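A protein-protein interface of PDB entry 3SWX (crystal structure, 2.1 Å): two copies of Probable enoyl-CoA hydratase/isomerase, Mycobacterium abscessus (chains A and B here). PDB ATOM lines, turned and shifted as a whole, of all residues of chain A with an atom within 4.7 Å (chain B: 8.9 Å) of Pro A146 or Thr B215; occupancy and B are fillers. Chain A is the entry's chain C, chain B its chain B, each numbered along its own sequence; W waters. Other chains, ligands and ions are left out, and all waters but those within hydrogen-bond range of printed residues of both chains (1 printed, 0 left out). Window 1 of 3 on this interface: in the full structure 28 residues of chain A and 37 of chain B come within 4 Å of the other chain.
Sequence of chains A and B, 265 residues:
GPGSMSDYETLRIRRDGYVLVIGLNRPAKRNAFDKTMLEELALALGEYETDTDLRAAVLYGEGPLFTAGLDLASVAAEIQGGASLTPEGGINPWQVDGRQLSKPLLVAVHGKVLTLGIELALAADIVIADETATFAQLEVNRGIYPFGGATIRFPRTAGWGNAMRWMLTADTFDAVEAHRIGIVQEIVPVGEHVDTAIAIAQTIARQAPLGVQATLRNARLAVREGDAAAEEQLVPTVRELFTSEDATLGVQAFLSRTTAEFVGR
The side-chain hydroxyl (OG1) of Thr A151 is in hydrogen-bond range of the side-chain amide oxygen (OD1) of Asn B218.
The backbone NH (N) of Ala B208 sits at hydrogen-bond distance from the backbone carbonyl oxygen (O) of Val A140, at 3.1 Å.
The backbone carbonyl oxygen (O) of Leu B234 sits at hydrogen-bond distance from the side-chain hydroxyl (OH) of Tyr A145 (2.8 Å).
The backbone carbonyl oxygen of Ala B230 sits at hydrogen-bond distance from the side-chain amide nitrogen of Asn B218 (3.1 Å).
O of Gln B233 is in hydrogen-bond range of OG1 of Thr B237 (2.7 Å).
The backbone carbonyl oxygen (O) of Gly B211 lies within hydrogen-bond range of the side-chain hydroxyl (OG1) of Thr B215, at 2.8 Å.
Gly B211 touches Val A140 (C to CG1, 3.6 Å).
Val A140 touches Val B212.
Tyr A145 touches Gly B211 (CB to O, 3.4 Å).
Tyr A145 touches Thr B215 (CB to OG1, 3.6 Å).
Tyr A145 touches Gln B233 (OH to O, 3.9 Å).
Tyr A145 touches Thr B237 (OH to CB, 3.5 Å).
Val B238 touches Tyr A145.
Thr B215 touches Pro A146 (OG1 to CD, 3.4 Å).
CG1 of Val B212 touches CD2 of Leu A168, 3.96 Å away.
CD2 of Leu A168 touches CG2 of Thr B215, 3.8 Å away.
Of chain B, only Gly B211 (3.4 Å), Ala B214 (3.9 Å), Thr B215 (3.6 Å), Gln B233 (3.9 Å), Leu B234 (2.8 Å), Thr B237 (3.5 Å), Val B238 (3.9 Å) and Leu B241 (3.6 Å) come within 4 Å of Tyr A145.
Pro A146 touches just one residue of chain B: Thr B215 (3.4 Å).
Ala A150 touches none of the printed residues of chain B.
Of the printed residues of chain B, Thr A151 touches Thr B215, Asn B218, Ala B219 and Leu B234.
Printed residues of chain A within 4 Å of Gln B207: Val A140 (3.7 Å) and Leu A168 (3.7 Å).
Printed residues of chain A within 4 Å of Thr B215: Val A140, Tyr A145, Pro A146, Thr A151 and Leu A168.
Printed residues of chain A within 4 Å of Leu B216: Met A164 (3.996 Å).
Printed residues of chain A within 4 Å of Gln B233: Tyr A145 (3.9 Å).
Of the printed residues of chain A, Val B238 touches Tyr A145 (3.9 Å) and Phe A147 (3.7 Å).
The nearest residue of chain B that does not touch Pro A146 is Leu B234 (4.5 Å).
The nearest printed residue of chain A that does not touch Thr B215 is Met A167 (4.0005 Å).
Of the 13 printed residues of chain A, 7 touch a printed residue of chain B.
Hydrophobic or aromatic side chains of chain A that line the printed part of chain B: Val A140, Tyr A145, Pro A146, Phe A147, Met A164 and Leu A168.
Among the printed residues, 26 pairs touch across the chains.
No position is printed for both chains.
Of the 26 pairs that touch across the chains among the printed residues, none has its exchanged pair printed and touching as well.
Water W1 lies within hydrogen-bond range of O of Ala B219 (2.7 Å) and O of Thr A151 (2.8 Å).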
ATOM      1  N   GLU A 119     -31.774  -2.885 -10.439  1.00  0.00           N
ATOM      2  CA  GLU A 119     -31.729  -2.263 -11.767  1.00  0.00           C
ATOM      3  C   GLU A 119     -33.099  -2.165 -12.451  1.00  0.00           C
ATOM      4  O   GLU A 119     -33.349  -1.212 -13.192  1.00  0.00           O
ATOM      5  CB  GLU A 119     -30.683  -2.921 -12.632  1.00  0.00           C
ATOM      6  CG  GLU A 119     -29.289  -2.672 -12.114  1.00  0.00           C
ATOM      7  CD  GLU A 119     -28.246  -3.521 -12.813  1.00  0.00           C
ATOM      8  OE1 GLU A 119     -27.204  -2.957 -13.222  1.00  0.00           O
ATOM      9  OE2 GLU A 119     -28.468  -4.752 -12.964  1.00  0.00           O
ATOM     10  N   GLN A 137     -26.287  -4.894  -4.181  1.00  0.00           N
ATOM     11  CA  GLN A 137     -25.684  -4.845  -5.494  1.00  0.00           C
ATOM     12  C   GLN A 137     -24.493  -5.804  -5.463  1.00  0.00           C
ATOM     13  O   GLN A 137     -23.336  -5.393  -5.361  1.00  0.00           O
ATOM     14  CB  GLN A 137     -25.272  -3.405  -5.818  1.00  0.00           C
ATOM     15  CG  GLN A 137     -25.070  -3.145  -7.292  1.00  0.00           C
ATOM     16  CD  GLN A 137     -26.390  -2.903  -8.035  1.00  0.00           C
ATOM     17  OE1 GLN A 137     -27.035  -1.841  -7.899  1.00  0.00           O
ATOM     18  NE2 GLN A 137     -26.782  -3.879  -8.828  1.00  0.00           N
ATOM     19  N   GLU A 139     -23.077  -7.886  -7.584  1.00  0.00           N
ATOM     20  CA  GLU A 139     -22.343  -8.279  -8.800  1.00  0.00           C
ATOM     21  C   GLU A 139     -20.818  -8.299  -8.602  1.00  0.00           C
ATOM     22  O   GLU A 139     -20.161  -9.259  -9.018  1.00  0.00           O
ATOM     23  CB  GLU A 139     -22.714  -7.404  -9.997  1.00  0.00           C
ATOM     24  CG  GLU A 139     -24.158  -7.528 -10.522  1.00  0.00           C
ATOM     25  CD  GLU A 139     -25.126  -6.548  -9.893  1.00  0.00           C
ATOM     26  OE1 GLU A 139     -24.959  -6.166  -8.711  1.00  0.00           O
ATOM     27  OE2 GLU A 139     -26.079  -6.156 -10.581  1.00  0.00           O
ATOM     28  N   VAL A 140     -20.249  -7.287  -7.940  1.00  0.00           N
ATOM     29  CA  VAL A 140     -18.810  -7.324  -7.686  1.00  0.00           C
ATOM     30  C   VAL A 140     -18.420  -8.437  -6.703  1.00  0.00           C
ATOM     31  O   VAL A 140     -17.271  -8.857  -6.703  1.00  0.00           O
ATOM     32  CB  VAL A 140     -18.214  -5.951  -7.224  1.00  0.00           C
ATOM     33  CG1 VAL A 140     -18.392  -4.879  -8.332  1.00  0.00           C
ATOM     34  CG2 VAL A 140     -18.784  -5.501  -5.858  1.00  0.00           C
ATOM     35  N   TYR A 145     -19.861  -7.208 -12.530  1.00  0.00           N
ATOM     36  CA  TYR A 145     -20.211  -5.843 -12.111  1.00  0.00           C
ATOM     37  C   TYR A 145     -21.654  -5.593 -12.536  1.00  0.00           C
ATOM     38  O   TYR A 145     -22.218  -6.436 -13.235  1.00  0.00           O
ATOM     39  CB  TYR A 145     -19.261  -4.821 -12.721  1.00  0.00           C
ATOM     40  CG  TYR A 145     -19.673  -4.368 -14.111  1.00  0.00           C
ATOM     41  CD1 TYR A 145     -19.861  -5.295 -15.129  1.00  0.00           C
ATOM     42  CD2 TYR A 145     -19.857  -3.017 -14.407  1.00  0.00           C
ATOM     43  CE1 TYR A 145     -20.220  -4.899 -16.413  1.00  0.00           C
ATOM     44  CE2 TYR A 145     -20.223  -2.614 -15.685  1.00  0.00           C
ATOM     45  CZ  TYR A 145     -20.413  -3.576 -16.678  1.00  0.00           C
ATOM     46  OH  TYR A 145     -20.774  -3.226 -17.946  1.00  0.00           O
ATOM     47  N   PRO A 146     -22.262  -4.469 -12.115  1.00  0.00           N
ATOM     48  CA  PRO A 146     -23.664  -4.258 -12.496  1.00  0.00           C
ATOM     49  C   PRO A 146     -23.806  -3.846 -13.945  1.00  0.00           C
ATOM     50  O   PRO A 146     -23.364  -2.757 -14.309  1.00  0.00           O
ATOM     51  CB  PRO A 146     -24.127  -3.124 -11.574  1.00  0.00           C
ATOM     52  CG  PRO A 146     -23.067  -3.012 -10.518  1.00  0.00           C
ATOM     53  CD  PRO A 146     -21.807  -3.470 -11.137  1.00  0.00           C
ATOM     54  N   PHE A 147     -24.438  -4.686 -14.759  1.00  0.00           N
ATOM     55  CA  PHE A 147     -24.487  -4.432 -16.203  1.00  0.00           C
ATOM     56  C   PHE A 147     -25.906  -4.219 -16.715  1.00  0.00           C
ATOM     57  O   PHE A 147     -26.148  -4.262 -17.923  1.00  0.00           O
ATOM     58  CB  PHE A 147     -23.739  -5.516 -16.997  1.00  0.00           C
ATOM     59  CG  PHE A 147     -24.344  -6.878 -16.904  1.00  0.00           C
ATOM     60  CD1 PHE A 147     -25.096  -7.384 -17.946  1.00  0.00           C
ATOM     61  CD2 PHE A 147     -24.127  -7.673 -15.788  1.00  0.00           C
ATOM     62  CE1 PHE A 147     -25.654  -8.666 -17.867  1.00  0.00           C
ATOM     63  CE2 PHE A 147     -24.687  -8.954 -15.688  1.00  0.00           C
ATOM     64  CZ  PHE A 147     -25.448  -9.446 -16.729  1.00  0.00           C
ATOM     65  N   GLY A 148     -26.819  -3.920 -15.804  1.00  0.00           N
ATOM     66  CA  GLY A 148     -28.216  -3.663 -16.168  1.00  0.00           C
ATOM     67  C   GLY A 148     -28.630  -2.211 -16.009  1.00  0.00           C
ATOM     68  O   GLY A 148     -29.833  -1.895 -15.951  1.00  0.00           O
ATOM     69  N   ALA A 150     -27.412   0.032 -13.483  1.00  0.00           N
ATOM     70  CA  ALA A 150     -27.088   0.675 -12.195  1.00  0.00           C
ATOM     71  C   ALA A 150     -25.909   1.677 -12.309  1.00  0.00           C
ATOM     72  O   ALA A 150     -25.889   2.709 -11.639  1.00  0.00           O
ATOM     73  CB  ALA A 150     -26.791  -0.364 -11.107  1.00  0.00           C
ATOM     74  N   THR A 151     -24.935   1.393 -13.165  1.00  0.00           N
ATOM     75  CA  THR A 151     -23.775   2.304 -13.292  1.00  0.00           C
ATOM     76  C   THR A 151     -24.141   3.681 -13.839  1.00  0.00           C
ATOM     77  O   THR A 151     -23.448   4.663 -13.593  1.00  0.00           O
ATOM     78  CB  THR A 151     -22.668   1.719 -14.200  1.00  0.00           C
ATOM     79  OG1 THR A 151     -23.237   1.337 -15.470  1.00  0.00           O
ATOM     80  CG2 THR A 151     -22.015   0.511 -13.535  1.00  0.00           C
ATOM     81  N   MET A 164     -22.030   4.727  -5.078  1.00  0.00           N
ATOM     82  CA  MET A 164     -20.809   3.939  -4.967  1.00  0.00           C
ATOM     83  C   MET A 164     -20.660   3.214  -3.616  1.00  0.00           C
ATOM     84  O   MET A 164     -20.085   2.125  -3.566  1.00  0.00           O
ATOM     85  CB  MET A 164     -19.598   4.815  -5.267  1.00  0.00           C
ATOM     86  CG  MET A 164     -19.557   5.293  -6.711  1.00  0.00           C
ATOM     87  SD  MET A 164     -19.400   3.888  -7.854  1.00  0.00           S
ATOM     88  CE  MET A 164     -19.830   4.655  -9.426  1.00  0.00           C
ATOM     89  N   MET A 167     -22.693   0.094  -4.581  1.00  0.00           N
ATOM     90  CA  MET A 167     -22.213  -0.630  -5.763  1.00  0.00           C
ATOM     91  C   MET A 167     -20.794  -1.173  -5.624  1.00  0.00           C
ATOM     92  O   MET A 167     -20.479  -2.204  -6.180  1.00  0.00           O
ATOM     93  CB  MET A 167     -22.318   0.226  -7.034  1.00  0.00           C
ATOM     94  CG  MET A 167     -23.753   0.627  -7.442  1.00  0.00           C
ATOM     95  SD  MET A 167     -23.807   1.298  -9.143  1.00  0.00           S
ATOM     96  CE  MET A 167     -22.627   2.652  -9.101  1.00  0.00           C
ATOM     97  N   LEU A 168     -19.922  -0.483  -4.902  1.00  0.00           N
ATOM     98  CA  LEU A 168     -18.525  -0.916  -4.856  1.00  0.00           C
ATOM     99  C   LEU A 168     -18.295  -1.965  -3.757  1.00  0.00           C
ATOM    100  O   LEU A 168     -17.289  -2.696  -3.779  1.00  0.00           O
ATOM    101  CB  LEU A 168     -17.585   0.289  -4.648  1.00  0.00           C
ATOM    102  CG  LEU A 168     -17.536   1.371  -5.735  1.00  0.00           C
ATOM    103  CD1 LEU A 168     -16.544   2.490  -5.350  1.00  0.00           C
ATOM    104  CD2 LEU A 168     -17.177   0.767  -7.117  1.00  0.00           C
ATOM    105  N   LEU B 101      -9.143   8.790 -11.256  1.00  0.00           N
ATOM    106  CA  LEU B 101      -8.694   7.518 -10.670  1.00  0.00           C
ATOM    107  C   LEU B 101      -9.499   6.312 -11.164  1.00  0.00           C
ATOM    108  O   LEU B 101     -10.733   6.370 -11.271  1.00  0.00           O
ATOM    109  CB  LEU B 101      -8.769   7.571  -9.143  1.00  0.00           C
ATOM    110  CG  LEU B 101      -7.764   8.501  -8.458  1.00  0.00           C
ATOM    111  CD1 LEU B 101      -8.008   8.530  -6.947  1.00  0.00           C
ATOM    112  CD2 LEU B 101      -6.316   8.053  -8.800  1.00  0.00           C
ATOM    113  N   SER B 102      -8.786   5.220 -11.426  1.00  0.00           N
ATOM    114  CA  SER B 102      -9.377   3.970 -11.925  1.00  0.00           C
ATOM    115  C   SER B 102      -9.855   3.097 -10.802  1.00  0.00           C
ATOM    116  O   SER B 102     -10.538   2.105 -11.039  1.00  0.00           O
ATOM    117  CB  SER B 102      -8.332   3.155 -12.709  1.00  0.00           C
ATOM    118  OG  SER B 102      -7.958   3.836 -13.886  1.00  0.00           O
ATOM    119  N   PRO B 104     -10.993   2.955  -6.316  1.00  0.00           N
ATOM    120  CA  PRO B 104     -11.785   3.736  -5.365  1.00  0.00           C
ATOM    121  C   PRO B 104     -10.977   4.648  -4.455  1.00  0.00           C
ATOM    122  O   PRO B 104      -9.861   4.310  -4.068  1.00  0.00           O
ATOM    123  CB  PRO B 104     -12.528   2.662  -4.571  1.00  0.00           C
ATOM    124  CG  PRO B 104     -12.583   1.489  -5.480  1.00  0.00           C
ATOM    125  CD  PRO B 104     -11.260   1.513  -6.175  1.00  0.00           C
ATOM    126  N   ASP B 125     -15.162   8.770  -4.057  1.00  0.00           N
ATOM    127  CA  ASP B 125     -16.291   7.886  -4.307  1.00  0.00           C
ATOM    128  C   ASP B 125     -17.177   7.706  -3.095  1.00  0.00           C
ATOM    129  O   ASP B 125     -18.364   7.472  -3.244  1.00  0.00           O
ATOM    130  CB  ASP B 125     -15.790   6.537  -4.828  1.00  0.00           C
ATOM    131  CG  ASP B 125     -14.921   6.700  -6.028  1.00  0.00           C
ATOM    132  OD1 ASP B 125     -15.421   7.289  -7.022  1.00  0.00           O
ATOM    133  OD2 ASP B 125     -13.733   6.318  -5.955  1.00  0.00           O
ATOM    134  N   GLN B 207     -13.991  -7.526  -2.673  1.00  0.00           N
ATOM    135  CA  GLN B 207     -14.728  -7.740  -3.917  1.00  0.00           C
ATOM    136  C   GLN B 207     -13.763  -7.872  -5.098  1.00  0.00           C
ATOM    137  O   GLN B 207     -12.556  -7.625  -4.971  1.00  0.00           O
ATOM    138  CB  GLN B 207     -15.720  -6.604  -4.149  1.00  0.00           C
ATOM    139  CG  GLN B 207     -16.457  -6.187  -2.869  1.00  0.00           C
ATOM    140  CD  GLN B 207     -17.116  -7.356  -2.158  1.00  0.00           C
ATOM    141  OE1 GLN B 207     -17.774  -8.188  -2.788  1.00  0.00           O
ATOM    142  NE2 GLN B 207     -16.957  -7.415  -0.845  1.00  0.00           N
ATOM    143  N   ALA B 208     -14.297  -8.274  -6.244  1.00  0.00           N
ATOM    144  CA  ALA B 208     -13.456  -8.539  -7.413  1.00  0.00           C
ATOM    145  C   ALA B 208     -12.966  -7.228  -8.003  1.00  0.00           C
ATOM    146  O   ALA B 208     -13.788  -6.470  -8.505  1.00  0.00           O
ATOM    147  CB  ALA B 208     -14.242  -9.319  -8.453  1.00  0.00           C
ATOM    148  N   PRO B 209     -11.630  -6.953  -7.945  1.00  0.00           N
ATOM    149  CA  PRO B 209     -11.086  -5.682  -8.397  1.00  0.00           C
ATOM    150  C   PRO B 209     -11.471  -5.244  -9.822  1.00  0.00           C
ATOM    151  O   PRO B 209     -11.743  -4.060 -10.019  1.00  0.00           O
ATOM    152  CB  PRO B 209      -9.562  -5.880  -8.319  1.00  0.00           C
ATOM    153  CG  PRO B 209      -9.361  -6.928  -7.287  1.00  0.00           C
ATOM    154  CD  PRO B 209     -10.569  -7.829  -7.405  1.00  0.00           C
ATOM    155  N   LEU B 210     -11.485  -6.158 -10.794  1.00  0.00           N
ATOM    156  CA  LEU B 210     -11.810  -5.770 -12.175  1.00  0.00           C
ATOM    157  C   LEU B 210     -13.291  -5.374 -12.288  1.00  0.00           C
ATOM    158  O   LEU B 210     -13.664  -4.577 -13.130  1.00  0.00           O
ATOM    159  CB  LEU B 210     -11.497  -6.908 -13.165  1.00  0.00           C
ATOM    160  CG  LEU B 210     -10.063  -7.425 -13.260  1.00  0.00           C
ATOM    161  CD1 LEU B 210     -10.006  -8.533 -14.317  1.00  0.00           C
ATOM    162  CD2 LEU B 210      -9.051  -6.318 -13.562  1.00  0.00           C
ATOM    163  N   GLY B 211     -14.123  -5.953 -11.436  1.00  0.00           N
ATOM    164  CA  GLY B 211     -15.546  -5.589 -11.361  1.00  0.00           C
ATOM    165  C   GLY B 211     -15.720  -4.221 -10.729  1.00  0.00           C
ATOM    166  O   GLY B 211     -16.535  -3.430 -11.175  1.00  0.00           O
ATOM    167  N   VAL B 212     -14.950  -3.960  -9.672  1.00  0.00           N
ATOM    168  CA  VAL B 212     -14.933  -2.648  -9.020  1.00  0.00           C
ATOM    169  C   VAL B 212     -14.492  -1.607 -10.060  1.00  0.00           C
ATOM    170  O   VAL B 212     -15.122  -0.568 -10.237  1.00  0.00           O
ATOM    171  CB  VAL B 212     -14.012  -2.673  -7.742  1.00  0.00           C
ATOM    172  CG1 VAL B 212     -13.785  -1.267  -7.162  1.00  0.00           C
ATOM    173  CG2 VAL B 212     -14.590  -3.627  -6.664  1.00  0.00           C
ATOM    174  N   GLN B 213     -13.435  -1.931 -10.792  1.00  0.00           N
ATOM    175  CA  GLN B 213     -12.874  -1.021 -11.787  1.00  0.00           C
ATOM    176  C   GLN B 213     -13.851  -0.764 -12.910  1.00  0.00           C
ATOM    177  O   GLN B 213     -14.029   0.390 -13.325  1.00  0.00           O
ATOM    178  CB  GLN B 213     -11.564  -1.557 -12.335  1.00  0.00           C
ATOM    179  CG  GLN B 213     -10.410  -1.453 -11.342  1.00  0.00           C
ATOM    180  CD  GLN B 213      -9.157  -2.094 -11.880  1.00  0.00           C
ATOM    181  OE1 GLN B 213      -8.950  -2.130 -13.099  1.00  0.00           O
ATOM    182  NE2 GLN B 213      -8.300  -2.581 -10.985  1.00  0.00           N
ATOM    183  N   ALA B 214     -14.506  -1.825 -13.368  1.00  0.00           N
ATOM    184  CA  ALA B 214     -15.536  -1.710 -14.413  1.00  0.00           C
ATOM    185  C   ALA B 214     -16.714  -0.830 -13.958  1.00  0.00           C
ATOM    186  O   ALA B 214     -17.253  -0.065 -14.728  1.00  0.00           O
ATOM    187  CB  ALA B 214     -16.023  -3.116 -14.864  1.00  0.00           C
ATOM    188  N   THR B 215     -17.128  -0.980 -12.708  1.00  0.00           N
ATOM    189  CA  THR B 215     -18.182  -0.145 -12.122  1.00  0.00           C
ATOM    190  C   THR B 215     -17.839   1.367 -12.198  1.00  0.00           C
ATOM    191  O   THR B 215     -18.653   2.195 -12.648  1.00  0.00           O
ATOM    192  CB  THR B 215     -18.455  -0.572 -10.651  1.00  0.00           C
ATOM    193  OG1 THR B 215     -18.817  -1.967 -10.607  1.00  0.00           O
ATOM    194  CG2 THR B 215     -19.585   0.239 -10.064  1.00  0.00           C
ATOM    195  N   LEU B 216     -16.624   1.713 -11.791  1.00  0.00           N
ATOM    196  CA  LEU B 216     -16.149   3.081 -11.833  1.00  0.00           C
ATOM    197  C   LEU B 216     -16.031   3.557 -13.274  1.00  0.00           C
ATOM    198  O   LEU B 216     -16.472   4.640 -13.579  1.00  0.00           O
ATOM    199  CB  LEU B 216     -14.794   3.219 -11.106  1.00  0.00           C
ATOM    200  CG  LEU B 216     -14.840   3.172  -9.578  1.00  0.00           C
ATOM    201  CD1 LEU B 216     -13.448   3.159  -8.987  1.00  0.00           C
ATOM    202  CD2 LEU B 216     -15.616   4.368  -9.045  1.00  0.00           C
ATOM    203  N   ARG B 217     -15.471   2.718 -14.148  1.00  0.00           N
ATOM    204  CA  ARG B 217     -15.228   3.076 -15.546  1.00  0.00           C
ATOM    205  C   ARG B 217     -16.527   3.357 -16.306  1.00  0.00           C
ATOM    206  O   ARG B 217     -16.660   4.391 -16.967  1.00  0.00           O
ATOM    207  CB  ARG B 217     -14.394   1.983 -16.255  1.00  0.00           C
ATOM    208  CG  ARG B 217     -13.958   2.340 -17.698  1.00  0.00           C
ATOM    209  CD  ARG B 217     -12.938   1.346 -18.283  1.00  0.00           C
ATOM    210  NE  ARG B 217     -13.463  -0.019 -18.345  1.00  0.00           N
ATOM    211  CZ  ARG B 217     -13.108  -1.034 -17.553  1.00  0.00           C
ATOM    212  NH1 ARG B 217     -12.197  -0.896 -16.592  1.00  0.00           N
ATOM    213  NH2 ARG B 217     -13.694  -2.211 -17.726  1.00  0.00           N
ATOM    214  N   ASN B 218     -17.495   2.463 -16.206  1.00  0.00           N
ATOM    215  CA  ASN B 218     -18.725   2.663 -16.936  1.00  0.00           C
ATOM    216  C   ASN B 218     -19.518   3.853 -16.387  1.00  0.00           C
ATOM    217  O   ASN B 218     -20.093   4.613 -17.161  1.00  0.00           O
ATOM    218  CB  ASN B 218     -19.563   1.400 -16.928  1.00  0.00           C
ATOM    219  CG  ASN B 218     -20.684   1.458 -17.922  1.00  0.00           C
ATOM    220  OD1 ASN B 218     -21.815   1.843 -17.588  1.00  0.00           O
ATOM    221  ND2 ASN B 218     -20.375   1.098 -19.176  1.00  0.00           N
ATOM    222  N   ALA B 219     -19.550   3.993 -15.053  1.00  0.00           N
ATOM    223  CA  ALA B 219     -20.199   5.123 -14.409  1.00  0.00           C
ATOM    224  C   ALA B 219     -19.601   6.454 -14.893  1.00  0.00           C
ATOM    225  O   ALA B 219     -20.348   7.390 -15.204  1.00  0.00           O
ATOM    226  CB  ALA B 219     -20.094   5.014 -12.864  1.00  0.00           C
ATOM    227  N   ARG B 220     -18.269   6.537 -14.961  1.00  0.00           N
ATOM    228  CA  ARG B 220     -17.624   7.756 -15.461  1.00  0.00           C
ATOM    229  C   ARG B 220     -17.906   8.034 -16.935  1.00  0.00           C
ATOM    230  O   ARG B 220     -18.093   9.177 -17.318  1.00  0.00           O
ATOM    231  CB  ARG B 220     -16.123   7.729 -15.260  1.00  0.00           C
ATOM    232  CG  ARG B 220     -15.673   7.814 -13.814  1.00  0.00           C
ATOM    233  CD  ARG B 220     -14.168   8.031 -13.771  1.00  0.00           C
ATOM    234  NE  ARG B 220     -13.553   7.588 -12.519  1.00  0.00           N
ATOM    235  CZ  ARG B 220     -13.679   8.187 -11.338  1.00  0.00           C
ATOM    236  NH1 ARG B 220     -14.427   9.267 -11.203  1.00  0.00           N
ATOM    237  NH2 ARG B 220     -13.034   7.697 -10.265  1.00  0.00           N
ATOM    238  N   LEU B 221     -17.908   6.983 -17.753  1.00  0.00           N
ATOM    239  CA  LEU B 221     -18.210   7.103 -19.188  1.00  0.00           C
ATOM    240  C   LEU B 221     -19.608   7.685 -19.399  1.00  0.00           C
ATOM    241  O   LEU B 221     -19.792   8.546 -20.254  1.00  0.00           O
ATOM    242  CB  LEU B 221     -18.096   5.749 -19.885  1.00  0.00           C
ATOM    243  CG  LEU B 221     -18.250   5.759 -21.414  1.00  0.00           C
ATOM    244  CD1 LEU B 221     -17.314   6.764 -22.034  1.00  0.00           C
ATOM    245  CD2 LEU B 221     -18.037   4.342 -21.996  1.00  0.00           C
ATOM    246  N   ALA B 222     -20.570   7.236 -18.586  1.00  0.00           N
ATOM    247  CA  ALA B 222     -21.940   7.756 -18.635  1.00  0.00           C
ATOM    248  C   ALA B 222     -21.991   9.267 -18.420  1.00  0.00           C
ATOM    249  O   ALA B 222     -22.731  10.002 -19.122  1.00  0.00           O
ATOM    250  CB  ALA B 222     -22.812   7.068 -17.583  1.00  0.00           C
ATOM    251  N   ALA B 230     -22.193   4.645 -22.410  1.00  0.00           N
ATOM    252  CA  ALA B 230     -22.098   3.683 -21.319  1.00  0.00           C
ATOM    253  C   ALA B 230     -22.880   2.397 -21.648  1.00  0.00           C
ATOM    254  O   ALA B 230     -22.373   1.281 -21.475  1.00  0.00           O
ATOM    255  CB  ALA B 230     -22.563   4.334 -19.991  1.00  0.00           C
ATOM    256  N   GLN B 233     -21.193  -0.172 -23.847  1.00  0.00           N
ATOM    257  CA  GLN B 233     -20.153  -0.957 -23.189  1.00  0.00           C
ATOM    258  C   GLN B 233     -20.661  -2.018 -22.196  1.00  0.00           C
ATOM    259  O   GLN B 233     -19.871  -2.833 -21.747  1.00  0.00           O
ATOM    260  CB  GLN B 233     -19.205  -0.023 -22.418  1.00  0.00           C
ATOM    261  CG  GLN B 233     -18.524   1.015 -23.252  1.00  0.00           C
ATOM    262  CD  GLN B 233     -17.659   0.417 -24.313  1.00  0.00           C
ATOM    263  OE1 GLN B 233     -17.247  -0.749 -24.214  1.00  0.00           O
ATOM    264  NE2 GLN B 233     -17.358   1.209 -25.346  1.00  0.00           N
ATOM    265  N   LEU B 234     -21.944  -2.000 -21.822  1.00  0.00           N
ATOM    266  CA  LEU B 234     -22.407  -2.827 -20.695  1.00  0.00           C
ATOM    267  C   LEU B 234     -22.155  -4.329 -20.892  1.00  0.00           C
ATOM    268  O   LEU B 234     -21.467  -4.963 -20.070  1.00  0.00           O
ATOM    269  CB  LEU B 234     -23.895  -2.597 -20.406  1.00  0.00           C
ATOM    270  CG  LEU B 234     -24.266  -1.230 -19.830  1.00  0.00           C
ATOM    271  CD1 LEU B 234     -25.772  -1.087 -19.811  1.00  0.00           C
ATOM    272  CD2 LEU B 234     -23.659  -1.039 -18.433  1.00  0.00           C
ATOM    273  N   VAL B 235     -22.684  -4.884 -21.980  1.00  0.00           N
ATOM    274  CA  VAL B 235     -22.535  -6.323 -22.259  1.00  0.00           C
ATOM    275  C   VAL B 235     -21.094  -6.676 -22.708  1.00  0.00           C
ATOM    276  O   VAL B 235     -20.545  -7.685 -22.260  1.00  0.00           O
ATOM    277  CB  VAL B 235     -23.598  -6.845 -23.293  1.00  0.00           C
ATOM    278  CG1 VAL B 235     -23.378  -8.339 -23.638  1.00  0.00           C
ATOM    279  CG2 VAL B 235     -25.026  -6.623 -22.778  1.00  0.00           C
ATOM    280  N   THR B 237     -18.350  -5.349 -21.689  1.00  0.00           N
ATOM    281  CA  THR B 237     -17.591  -5.360 -20.447  1.00  0.00           C
ATOM    282  C   THR B 237     -17.911  -6.589 -19.601  1.00  0.00           C
ATOM    283  O   THR B 237     -17.004  -7.214 -19.068  1.00  0.00           O
ATOM    284  CB  THR B 237     -17.833  -4.087 -19.664  1.00  0.00           C
ATOM    285  OG1 THR B 237     -17.454  -2.976 -20.481  1.00  0.00           O
ATOM    286  CG2 THR B 237     -17.038  -4.074 -18.330  1.00  0.00           C
ATOM    287  N   VAL B 238     -19.177  -6.982 -19.488  1.00  0.00           N
ATOM    288  CA  VAL B 238     -19.462  -8.175 -18.695  1.00  0.00           C
ATOM    289  C   VAL B 238     -18.924  -9.430 -19.361  1.00  0.00           C
ATOM    290  O   VAL B 238     -18.489 -10.356 -18.667  1.00  0.00           O
ATOM    291  CB  VAL B 238     -20.944  -8.361 -18.294  1.00  0.00           C
ATOM    292  CG1 VAL B 238     -21.762  -9.072 -19.401  1.00  0.00           C
ATOM    293  CG2 VAL B 238     -20.998  -9.134 -16.976  1.00  0.00           C
ATOM    294  N   LEU B 241     -15.300  -9.665 -18.460  1.00  0.00           N
ATOM    295  CA  LEU B 241     -15.151 -10.074 -17.062  1.00  0.00           C
ATOM    296  C   LEU B 241     -15.446 -11.572 -16.872  1.00  0.00           C
ATOM    297  O   LEU B 241     -14.736 -12.224 -16.132  1.00  0.00           O
ATOM    298  CB  LEU B 241     -16.030  -9.235 -16.129  1.00  0.00           C
ATOM    299  CG  LEU B 241     -15.637  -7.754 -15.976  1.00  0.00           C
ATOM    300  CD1 LEU B 241     -16.708  -7.018 -15.185  1.00  0.00           C
ATOM    301  CD2 LEU B 241     -14.269  -7.581 -15.344  1.00  0.00           C
HETATM  302  O   HOH W   1     -22.657   7.309 -13.759  1.00  0.00           O
